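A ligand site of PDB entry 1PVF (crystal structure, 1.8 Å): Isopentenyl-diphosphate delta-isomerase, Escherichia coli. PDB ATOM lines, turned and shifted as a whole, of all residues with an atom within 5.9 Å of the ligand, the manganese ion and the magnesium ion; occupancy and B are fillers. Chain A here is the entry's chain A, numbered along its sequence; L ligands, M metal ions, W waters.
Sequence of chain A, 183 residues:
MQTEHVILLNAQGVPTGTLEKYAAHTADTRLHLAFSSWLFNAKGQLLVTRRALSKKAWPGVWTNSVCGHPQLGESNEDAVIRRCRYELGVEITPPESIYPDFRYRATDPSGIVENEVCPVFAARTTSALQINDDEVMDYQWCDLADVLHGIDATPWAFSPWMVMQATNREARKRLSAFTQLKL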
ATOM      1  N   GLU A   4     -33.260   8.149  -8.724  1.00  0.00           N
ATOM      2  CA  GLU A   4     -32.874   8.777  -9.989  1.00  0.00           C
ATOM      3  C   GLU A   4     -33.353   7.978 -11.201  1.00  0.00           C
ATOM      4  O   GLU A   4     -33.609   6.768 -11.191  1.00  0.00           O
ATOM      5  CB  GLU A   4     -31.356   8.991 -10.044  1.00  0.00           C
ATOM      6  CG  GLU A   4     -30.936   9.841 -11.239  1.00  0.00           C
ATOM      7  CD  GLU A   4     -29.495  10.319 -11.123  1.00  0.00           C
ATOM      8  OE1 GLU A   4     -28.791   9.773 -10.245  1.00  0.00           O
ATOM      9  OE2 GLU A   4     -29.092  11.224 -11.893  1.00  0.00           O
ATOM     10  N   VAL A   6     -33.184   7.641 -15.823  1.00  0.00           N
ATOM     11  CA  VAL A   6     -32.685   8.126 -17.105  1.00  0.00           C
ATOM     12  C   VAL A   6     -33.925   8.395 -17.972  1.00  0.00           C
ATOM     13  O   VAL A   6     -35.006   7.855 -17.689  1.00  0.00           O
ATOM     14  CB  VAL A   6     -31.737   7.169 -17.823  1.00  0.00           C
ATOM     15  CG1 VAL A   6     -30.565   6.847 -16.877  1.00  0.00           C
ATOM     16  CG2 VAL A   6     -32.436   5.892 -18.250  1.00  0.00           C
ATOM     17  N   LYS A  21     -32.486   4.498 -12.842  1.00  0.00           N
ATOM     18  CA  LYS A  21     -31.167   4.560 -13.461  1.00  0.00           C
ATOM     19  C   LYS A  21     -30.427   3.234 -13.354  1.00  0.00           C
ATOM     20  O   LYS A  21     -29.881   2.725 -14.331  1.00  0.00           O
ATOM     21  CB  LYS A  21     -30.343   5.698 -12.858  1.00  0.00           C
ATOM     22  CG  LYS A  21     -28.991   5.921 -13.526  1.00  0.00           C
ATOM     23  CD  LYS A  21     -28.264   7.138 -12.938  1.00  0.00           C
ATOM     24  CE  LYS A  21     -27.609   6.734 -11.618  1.00  0.00           C
ATOM     25  NZ  LYS A  21     -26.977   7.902 -10.927  1.00  0.00           N
ATOM     26  N   HIS A  25     -29.194   0.357 -16.980  1.00  0.00           N
ATOM     27  CA  HIS A  25     -27.931  -0.014 -17.628  1.00  0.00           C
ATOM     28  C   HIS A  25     -27.724  -1.511 -17.506  1.00  0.00           C
ATOM     29  O   HIS A  25     -27.612  -2.053 -16.417  1.00  0.00           O
ATOM     30  CB  HIS A  25     -26.793   0.796 -16.984  1.00  0.00           C
ATOM     31  CG  HIS A  25     -26.938   2.277 -17.209  1.00  0.00           C
ATOM     32  ND1 HIS A  25     -27.659   3.091 -16.355  1.00  0.00           N
ATOM     33  CD2 HIS A  25     -26.493   3.084 -18.194  1.00  0.00           C
ATOM     34  CE1 HIS A  25     -27.614   4.330 -16.804  1.00  0.00           C
ATOM     35  NE2 HIS A  25     -26.914   4.362 -17.930  1.00  0.00           N
ATOM     36  N   THR A  29     -28.769  -2.032 -22.937  1.00  0.00           N
ATOM     37  CA  THR A  29     -29.210  -0.690 -22.607  1.00  0.00           C
ATOM     38  C   THR A  29     -29.855   0.045 -23.779  1.00  0.00           C
ATOM     39  O   THR A  29     -29.349   0.099 -24.893  1.00  0.00           O
ATOM     40  CB  THR A  29     -27.987   0.099 -22.113  1.00  0.00           C
ATOM     41  OG1 THR A  29     -27.514  -0.596 -20.944  1.00  0.00           O
ATOM     42  CG2 THR A  29     -28.350   1.516 -21.710  1.00  0.00           C
ATOM     43  N   HIS A  32     -30.653   6.582 -24.191  1.00  0.00           N
ATOM     44  CA  HIS A  32     -31.204   7.557 -23.250  1.00  0.00           C
ATOM     45  C   HIS A  32     -30.314   8.799 -23.172  1.00  0.00           C
ATOM     46  O   HIS A  32     -29.255   8.814 -23.795  1.00  0.00           O
ATOM     47  CB  HIS A  32     -31.372   6.907 -21.878  1.00  0.00           C
ATOM     48  CG  HIS A  32     -30.083   6.404 -21.305  1.00  0.00           C
ATOM     49  ND1 HIS A  32     -29.608   5.126 -21.546  1.00  0.00           N
ATOM     50  CD2 HIS A  32     -29.185   6.989 -20.470  1.00  0.00           C
ATOM     51  CE1 HIS A  32     -28.459   4.967 -20.901  1.00  0.00           C
ATOM     52  NE2 HIS A  32     -28.170   6.074 -20.226  1.00  0.00           N
ATOM     53  N   LEU A  33     -30.744   9.814 -22.439  1.00  0.00           N
ATOM     54  CA  LEU A  33     -30.039  11.089 -22.329  1.00  0.00           C
ATOM     55  C   LEU A  33     -28.936  11.047 -21.275  1.00  0.00           C
ATOM     56  O   LEU A  33     -29.122  10.476 -20.196  1.00  0.00           O
ATOM     57  CB  LEU A  33     -31.005  12.201 -21.930  1.00  0.00           C
ATOM     58  CG  LEU A  33     -30.549  13.637 -22.151  1.00  0.00           C
ATOM     59  CD1 LEU A  33     -29.891  13.842 -23.508  1.00  0.00           C
ATOM     60  CD2 LEU A  33     -31.751  14.570 -22.003  1.00  0.00           C
ATOM     61  N   ALA A  34     -27.817  11.693 -21.590  1.00  0.00           N
ATOM     62  CA  ALA A  34     -26.716  11.801 -20.633  1.00  0.00           C
ATOM     63  C   ALA A  34     -25.940  13.087 -20.887  1.00  0.00           C
ATOM     64  O   ALA A  34     -26.284  13.823 -21.808  1.00  0.00           O
ATOM     65  CB  ALA A  34     -25.806  10.599 -20.763  1.00  0.00           C
ATOM     66  N   PHE A  35     -24.912  13.359 -20.096  1.00  0.00           N
ATOM     67  CA  PHE A  35     -23.992  14.423 -20.401  1.00  0.00           C
ATOM     68  C   PHE A  35     -22.577  13.927 -20.087  1.00  0.00           C
ATOM     69  O   PHE A  35     -22.432  12.984 -19.305  1.00  0.00           O
ATOM     70  CB  PHE A  35     -24.229  15.708 -19.607  1.00  0.00           C
ATOM     71  CG  PHE A  35     -23.987  15.589 -18.115  1.00  0.00           C
ATOM     72  CD1 PHE A  35     -22.783  15.868 -17.478  1.00  0.00           C
ATOM     73  CD2 PHE A  35     -25.037  15.172 -17.315  1.00  0.00           C
ATOM     74  CE1 PHE A  35     -22.605  15.697 -16.123  1.00  0.00           C
ATOM     75  CE2 PHE A  35     -24.885  15.013 -15.949  1.00  0.00           C
ATOM     76  CZ  PHE A  35     -23.670  15.298 -15.347  1.00  0.00           C
ATOM     77  N   ARG A  51     -13.376   5.773 -12.021  1.00  0.00           N
ATOM     78  CA  ARG A  51     -14.703   5.376 -11.558  1.00  0.00           C
ATOM     79  C   ARG A  51     -14.616   4.335 -10.446  1.00  0.00           C
ATOM     80  O   ARG A  51     -13.803   3.430 -10.539  1.00  0.00           O
ATOM     81  CB  ARG A  51     -15.493   4.812 -12.742  1.00  0.00           C
ATOM     82  CG  ARG A  51     -15.843   5.884 -13.783  1.00  0.00           C
ATOM     83  CD  ARG A  51     -16.431   5.273 -15.045  1.00  0.00           C
ATOM     84  NE  ARG A  51     -17.724   4.628 -14.873  1.00  0.00           N
ATOM     85  CZ  ARG A  51     -18.872   5.269 -14.775  1.00  0.00           C
ATOM     86  NH1 ARG A  51     -18.890   6.599 -14.816  1.00  0.00           N
ATOM     87  NH2 ARG A  51     -20.032   4.626 -14.618  1.00  0.00           N
ATOM     88  N   LYS A  55     -19.370   1.157  -9.585  1.00  0.00           N
ATOM     89  CA  LYS A  55     -20.224   1.664 -10.672  1.00  0.00           C
ATOM     90  C   LYS A  55     -20.691   0.484 -11.524  1.00  0.00           C
ATOM     91  O   LYS A  55     -19.915  -0.447 -11.727  1.00  0.00           O
ATOM     92  CB  LYS A  55     -19.537   2.660 -11.591  1.00  0.00           C
ATOM     93  CG  LYS A  55     -19.131   3.978 -10.958  1.00  0.00           C
ATOM     94  CD  LYS A  55     -20.309   4.692 -10.322  1.00  0.00           C
ATOM     95  CE  LYS A  55     -21.276   5.239 -11.375  1.00  0.00           C
ATOM     96  NZ  LYS A  55     -22.347   6.000 -10.680  1.00  0.00           N
ATOM     97  N   ALA A  57     -21.429   0.467 -14.751  1.00  0.00           N
ATOM     98  CA  ALA A  57     -20.812   0.434 -16.070  1.00  0.00           C
ATOM     99  C   ALA A  57     -19.387   0.947 -15.975  1.00  0.00           C
ATOM    100  O   ALA A  57     -19.156   1.926 -15.262  1.00  0.00           O
ATOM    101  CB  ALA A  57     -21.599   1.289 -17.061  1.00  0.00           C
ATOM    102  N   VAL A  66     -16.503  14.102 -15.180  1.00  0.00           N
ATOM    103  CA  VAL A  66     -17.795  13.786 -14.612  1.00  0.00           C
ATOM    104  C   VAL A  66     -18.827  13.576 -15.719  1.00  0.00           C
ATOM    105  O   VAL A  66     -18.872  14.391 -16.642  1.00  0.00           O
ATOM    106  CB  VAL A  66     -18.297  14.899 -13.659  1.00  0.00           C
ATOM    107  CG1 VAL A  66     -18.116  16.269 -14.278  1.00  0.00           C
ATOM    108  CG2 VAL A  66     -19.763  14.658 -13.306  1.00  0.00           C
ATOM    109  N   CYS A  67     -19.573  12.489 -15.578  1.00  0.00           N
ATOM    110  CA  CYS A  67     -20.699  12.174 -16.440  1.00  0.00           C
ATOM    111  C   CYS A  67     -21.915  11.893 -15.564  1.00  0.00           C
ATOM    112  O   CYS A  67     -21.782  11.578 -14.376  1.00  0.00           O
ATOM    113  CB  CYS A  67     -20.452  10.971 -17.340  1.00  0.00           C
ATOM    114  SG  CYS A  67     -19.059  11.201 -18.468  1.00  0.00           S
ATOM    115  N   GLY A  68     -23.083  12.009 -16.180  1.00  0.00           N
ATOM    116  CA  GLY A  68     -24.303  11.760 -15.445  1.00  0.00           C
ATOM    117  C   GLY A  68     -25.503  11.756 -16.386  1.00  0.00           C
ATOM    118  O   GLY A  68     -25.335  11.668 -17.601  1.00  0.00           O
ATOM    119  N   HIS A  69     -26.673  11.818 -15.781  1.00  0.00           N
ATOM    120  CA  HIS A  69     -27.940  11.590 -16.480  1.00  0.00           C
ATOM    121  C   HIS A  69     -28.922  12.705 -16.120  1.00  0.00           C
ATOM    122  O   HIS A  69     -29.397  12.762 -14.996  1.00  0.00           O
ATOM    123  CB  HIS A  69     -28.464  10.203 -16.105  1.00  0.00           C
ATOM    124  CG  HIS A  69     -27.644   9.054 -16.601  1.00  0.00           C
ATOM    125  ND1 HIS A  69     -26.653   8.458 -15.836  1.00  0.00           N
ATOM    126  CD2 HIS A  69     -27.650   8.396 -17.782  1.00  0.00           C
ATOM    127  CE1 HIS A  69     -26.097   7.479 -16.534  1.00  0.00           C
ATOM    128  NE2 HIS A  69     -26.676   7.410 -17.718  1.00  0.00           N
ATOM    129  N   ARG A  83     -24.076  16.882 -10.676  1.00  0.00           N
ATOM    130  CA  ARG A  83     -23.234  15.706 -10.447  1.00  0.00           C
ATOM    131  C   ARG A  83     -21.854  16.135  -9.980  1.00  0.00           C
ATOM    132  O   ARG A  83     -21.154  15.349  -9.339  1.00  0.00           O
ATOM    133  CB  ARG A  83     -23.173  14.833 -11.701  1.00  0.00           C
ATOM    134  CG  ARG A  83     -24.501  14.119 -11.971  1.00  0.00           C
ATOM    135  CD  ARG A  83     -24.980  13.351 -10.762  1.00  0.00           C
ATOM    136  NE  ARG A  83     -24.194  12.125 -10.545  1.00  0.00           N
ATOM    137  CZ  ARG A  83     -24.595  11.186  -9.700  1.00  0.00           C
ATOM    138  NH1 ARG A  83     -25.736  11.384  -9.053  1.00  0.00           N
ATOM    139  NH2 ARG A  83     -23.897  10.071  -9.501  1.00  0.00           N
ATOM    140  N   GLU A  87     -20.617  14.024  -7.014  1.00  0.00           N
ATOM    141  CA  GLU A  87     -19.515  13.063  -7.137  1.00  0.00           C
ATOM    142  C   GLU A  87     -18.214  13.605  -6.562  1.00  0.00           C
ATOM    143  O   GLU A  87     -17.415  12.839  -6.021  1.00  0.00           O
ATOM    144  CB  GLU A  87     -19.304  12.687  -8.611  1.00  0.00           C
ATOM    145  CG  GLU A  87     -20.590  12.260  -9.307  1.00  0.00           C
ATOM    146  CD  GLU A  87     -20.323  11.674 -10.687  1.00  0.00           C
ATOM    147  OE1 GLU A  87     -19.150  11.667 -11.091  1.00  0.00           O
ATOM    148  OE2 GLU A  87     -21.281  11.243 -11.350  1.00  0.00           O
ATOM    149  N   GLU A 114     -23.436   1.184 -22.440  1.00  0.00           N
ATOM    150  CA  GLU A 114     -23.984   2.544 -22.371  1.00  0.00           C
ATOM    151  C   GLU A 114     -24.453   2.878 -23.795  1.00  0.00           C
ATOM    152  O   GLU A 114     -23.789   2.476 -24.751  1.00  0.00           O
ATOM    153  CB  GLU A 114     -23.043   3.655 -21.932  1.00  0.00           C
ATOM    154  CG  GLU A 114     -23.038   3.919 -20.432  1.00  0.00           C
ATOM    155  CD  GLU A 114     -24.291   4.582 -19.914  1.00  0.00           C
ATOM    156  OE1 GLU A 114     -24.206   5.107 -18.773  1.00  0.00           O
ATOM    157  OE2 GLU A 114     -25.342   4.589 -20.608  1.00  0.00           O
ATOM    158  N   ASN A 115     -25.559   3.590 -23.846  1.00  0.00           N
ATOM    159  CA  ASN A 115     -26.156   3.891 -25.159  1.00  0.00           C
ATOM    160  C   ASN A 115     -26.819   5.253 -25.004  1.00  0.00           C
ATOM    161  O   ASN A 115     -27.916   5.359 -24.449  1.00  0.00           O
ATOM    162  CB  ASN A 115     -27.118   2.781 -25.513  1.00  0.00           C
ATOM    163  CG  ASN A 115     -27.712   2.827 -26.905  1.00  0.00           C
ATOM    164  OD1 ASN A 115     -27.321   3.665 -27.713  1.00  0.00           O
ATOM    165  ND2 ASN A 115     -28.663   1.934 -27.180  1.00  0.00           N
ATOM    166  N   GLU A 116     -26.119   6.291 -25.451  1.00  0.00           N
ATOM    167  CA  GLU A 116     -26.490   7.610 -24.990  1.00  0.00           C
ATOM    168  C   GLU A 116     -26.368   8.688 -26.048  1.00  0.00           C
ATOM    169  O   GLU A 116     -25.510   8.700 -26.911  1.00  0.00           O
ATOM    170  CB  GLU A 116     -25.597   8.007 -23.791  1.00  0.00           C
ATOM    171  CG  GLU A 116     -25.982   7.292 -22.495  1.00  0.00           C
ATOM    172  CD  GLU A 116     -24.991   7.454 -21.350  1.00  0.00           C
ATOM    173  OE1 GLU A 116     -23.857   7.891 -21.640  1.00  0.00           O
ATOM    174  OE2 GLU A 116     -25.371   7.155 -20.189  1.00  0.00           O
ATOM    175  N   GLU A 135     -18.523   6.990  -5.940  1.00  0.00           N
ATOM    176  CA  GLU A 135     -18.500   7.352  -7.342  1.00  0.00           C
ATOM    177  C   GLU A 135     -17.098   7.365  -7.929  1.00  0.00           C
ATOM    178  O   GLU A 135     -16.886   6.986  -9.082  1.00  0.00           O
ATOM    179  CB  GLU A 135     -19.142   8.744  -7.538  1.00  0.00           C
ATOM    180  CG  GLU A 135     -20.583   8.824  -7.074  1.00  0.00           C
ATOM    181  CD  GLU A 135     -21.528   8.056  -7.978  1.00  0.00           C
ATOM    182  OE1 GLU A 135     -21.182   7.864  -9.158  1.00  0.00           O
ATOM    183  OE2 GLU A 135     -22.616   7.655  -7.514  1.00  0.00           O
ATOM    184  N   TRP A 161     -15.798   6.497 -24.284  1.00  0.00           N
ATOM    185  CA  TRP A 161     -16.349   7.832 -24.591  1.00  0.00           C
ATOM    186  C   TRP A 161     -15.324   8.934 -24.355  1.00  0.00           C
ATOM    187  O   TRP A 161     -15.295   9.927 -25.097  1.00  0.00           O
ATOM    188  CB  TRP A 161     -17.604   8.113 -23.760  1.00  0.00           C
ATOM    189  CG  TRP A 161     -17.392   8.246 -22.284  1.00  0.00           C
ATOM    190  CD1 TRP A 161     -17.052   9.350 -21.562  1.00  0.00           C
ATOM    191  CD2 TRP A 161     -17.542   7.173 -21.338  1.00  0.00           C
ATOM    192  NE1 TRP A 161     -16.964   9.035 -20.226  1.00  0.00           N
ATOM    193  CE2 TRP A 161     -17.262   7.714 -20.069  1.00  0.00           C
ATOM    194  CE3 TRP A 161     -17.877   5.827 -21.474  1.00  0.00           C
ATOM    195  CZ2 TRP A 161     -17.317   6.931 -18.912  1.00  0.00           C
ATOM    196  CZ3 TRP A 161     -17.931   5.052 -20.332  1.00  0.00           C
ATOM    197  CH2 TRP A 161     -17.644   5.609 -19.081  1.00  0.00           C
HETATM  198  P1  LIG L   1     -24.049   8.409 -13.162  1.00  0.00           P
HETATM  199  O1  LIG L   1     -25.305   8.954 -13.110  1.00  0.00           O
HETATM  200  O2  LIG L   1     -22.988   9.288 -12.557  1.00  0.00           O
HETATM  201  O3  LIG L   1     -24.115   7.160 -12.337  1.00  0.00           O
HETATM  202  O4  LIG L   1     -23.680   8.085 -14.589  1.00  0.00           O
HETATM  203  P2  LIG L   1     -22.356   7.764 -15.259  1.00  0.00           P
HETATM  204  O5  LIG L   1     -22.091   6.446 -15.279  1.00  0.00           O
HETATM  205  O6  LIG L   1     -21.327   8.584 -14.531  1.00  0.00           O
HETATM  206  O7  LIG L   1     -22.411   8.383 -16.657  1.00  0.00           O
HETATM  207 MN    MN M   1     -26.368   5.937 -19.189  1.00  0.00          MN
HETATM  208 MG    MG M   2     -21.223   9.942 -13.021  1.00  0.00          MG
HETATM  209  O   HOH W   1     -23.753   4.468 -16.054  1.00  0.00           O
HETATM  210  O   HOH W   2     -20.176   8.516 -11.677  1.00  0.00           O
HETATM  211  O   HOH W   3     -21.699   7.562 -19.023  1.00  0.00           O
HETATM  212  O   HOH W   4     -19.391  10.558 -13.416  1.00  0.00           O
HETATM  213  O   HOH W   5     -26.422  11.521 -13.095  1.00  0.00           O
HETATM  214  O   HOH W   6     -25.622   5.109 -13.985  1.00  0.00           O
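A ring nitrogen (ND1) of His 69 is in hydrogen-bond range of an oxygen (O1) of the ligand, at 3.1 Å.
NZ of Lys 55 lies within salt-bridge range of O3 of the ligand (2.7 Å).
NH2 of Arg 51 lies within salt-bridge range of O5 of the ligand (2.8 Å).
The side-chain amino group (NZ) of Lys 21 is in salt-bridge range of an oxygen (O1) of the ligand (2.9 Å).
An oxygen (O2) of the ligand lies close to the guanidinium group of Arg 83, 3.3 Å away.
The backbone carbonyl oxygen of Asn 115 is in hydrogen-bond range of the backbone NH of His 32 (3.0 Å).
A ring nitrogen (ND1) of His 25 lies within hydrogen-bond range of the backbone carbonyl oxygen of Lys 21, 3.0 Å away.
The side-chain carboxylate of Glu 87 sits close to the guanidinium group of Arg 83, at 3.1 Å.
SG of Cys 67 lies within hydrogen-bond range of NE1 of Trp 161 (3.5 Å).
NH2 of Arg 51 sits at hydrogen-bond distance from O of Ala 57 (2.9 Å).
The guanidinium group (NH2) of Arg 83 is in salt-bridge range of the side-chain carboxylate (OE2) of Glu 135 (3.4 Å).
NH1 of Arg 83 is in salt-bridge range of OE1 of Glu 4, 3.7 Å away.
O of Gly 68 is in hydrogen-bond range of N of Phe 35 (3.0 Å).
Merely in contact with the ligand: Gly 68 (3.7 Å).
Hydrophobic or aromatic side chains that line the ligand: His 69.
Eight residues have an atom within 4 Å of the ligand: Lys 21, Arg 51, Lys 55, Cys 67, Gly 68, His 69, Arg 83 and Glu 87.
Within 4 Å of the manganese ion: His 25, His 32, His 69, Glu 114 and Glu 116.
Along chain A the residues within 4 Å of the manganese ion span positions 25 to 116.
Two residues have an atom within 4 Å of the magnesium ion: Cys 67 and Glu 87.
The nearest printed residue that does not touch the magnesium ion is Gly 68 (4.2 Å).
The manganese ion is bound by the side-chain carboxylate (OE2) of Glu 116 (1.9 Å), a ring nitrogen (NE2) of His 32 (2.1 Å), a ring nitrogen (NE2) of His 25 (2.1 Å), a ring nitrogen (NE2) of His 69 (2.1 Å), the side-chain carboxylate (OE2) of Glu 114 (2.2 Å) and the side-chain carboxylate (OE1) of Glu 114 (2.4 Å).
The manganese ion has six donor atoms within binding distance.
The magnesium ion is bound by an oxygen (O2) of the ligand (1.9 Å), water W4 (2.0 Å), an oxygen (O6) of the ligand (2.0 Å), the side-chain carboxylate of Glu 87 (2.1 Å), the backbone carbonyl oxygen of Cys 67 (2.2 Å) and water W2 (2.2 Å).
The magnesium ion has six donor atoms within binding distance.
Water W4 lies within hydrogen-bond range of OE1 of Glu 87 and N of Cys 67.
Water W2 lies within hydrogen-bond range of OE1 of Glu 135 (2.8 Å), OE1 of Glu 87 (3.4 Å) and NZ of Lys 55 (3.5 Å).
Water W3 bridges O7 of the ligand (2.6 Å) and OE1 of Glu 116 (3.4 Å).
Water W5 lies within hydrogen-bond range of the backbone NH of His 69 (2.7 Å), an oxygen (O1) of the ligand (2.8 Å), the side-chain carboxylate of Glu 4 (2.9 Å) and the guanidinium group of Arg 83 (3.4 Å).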
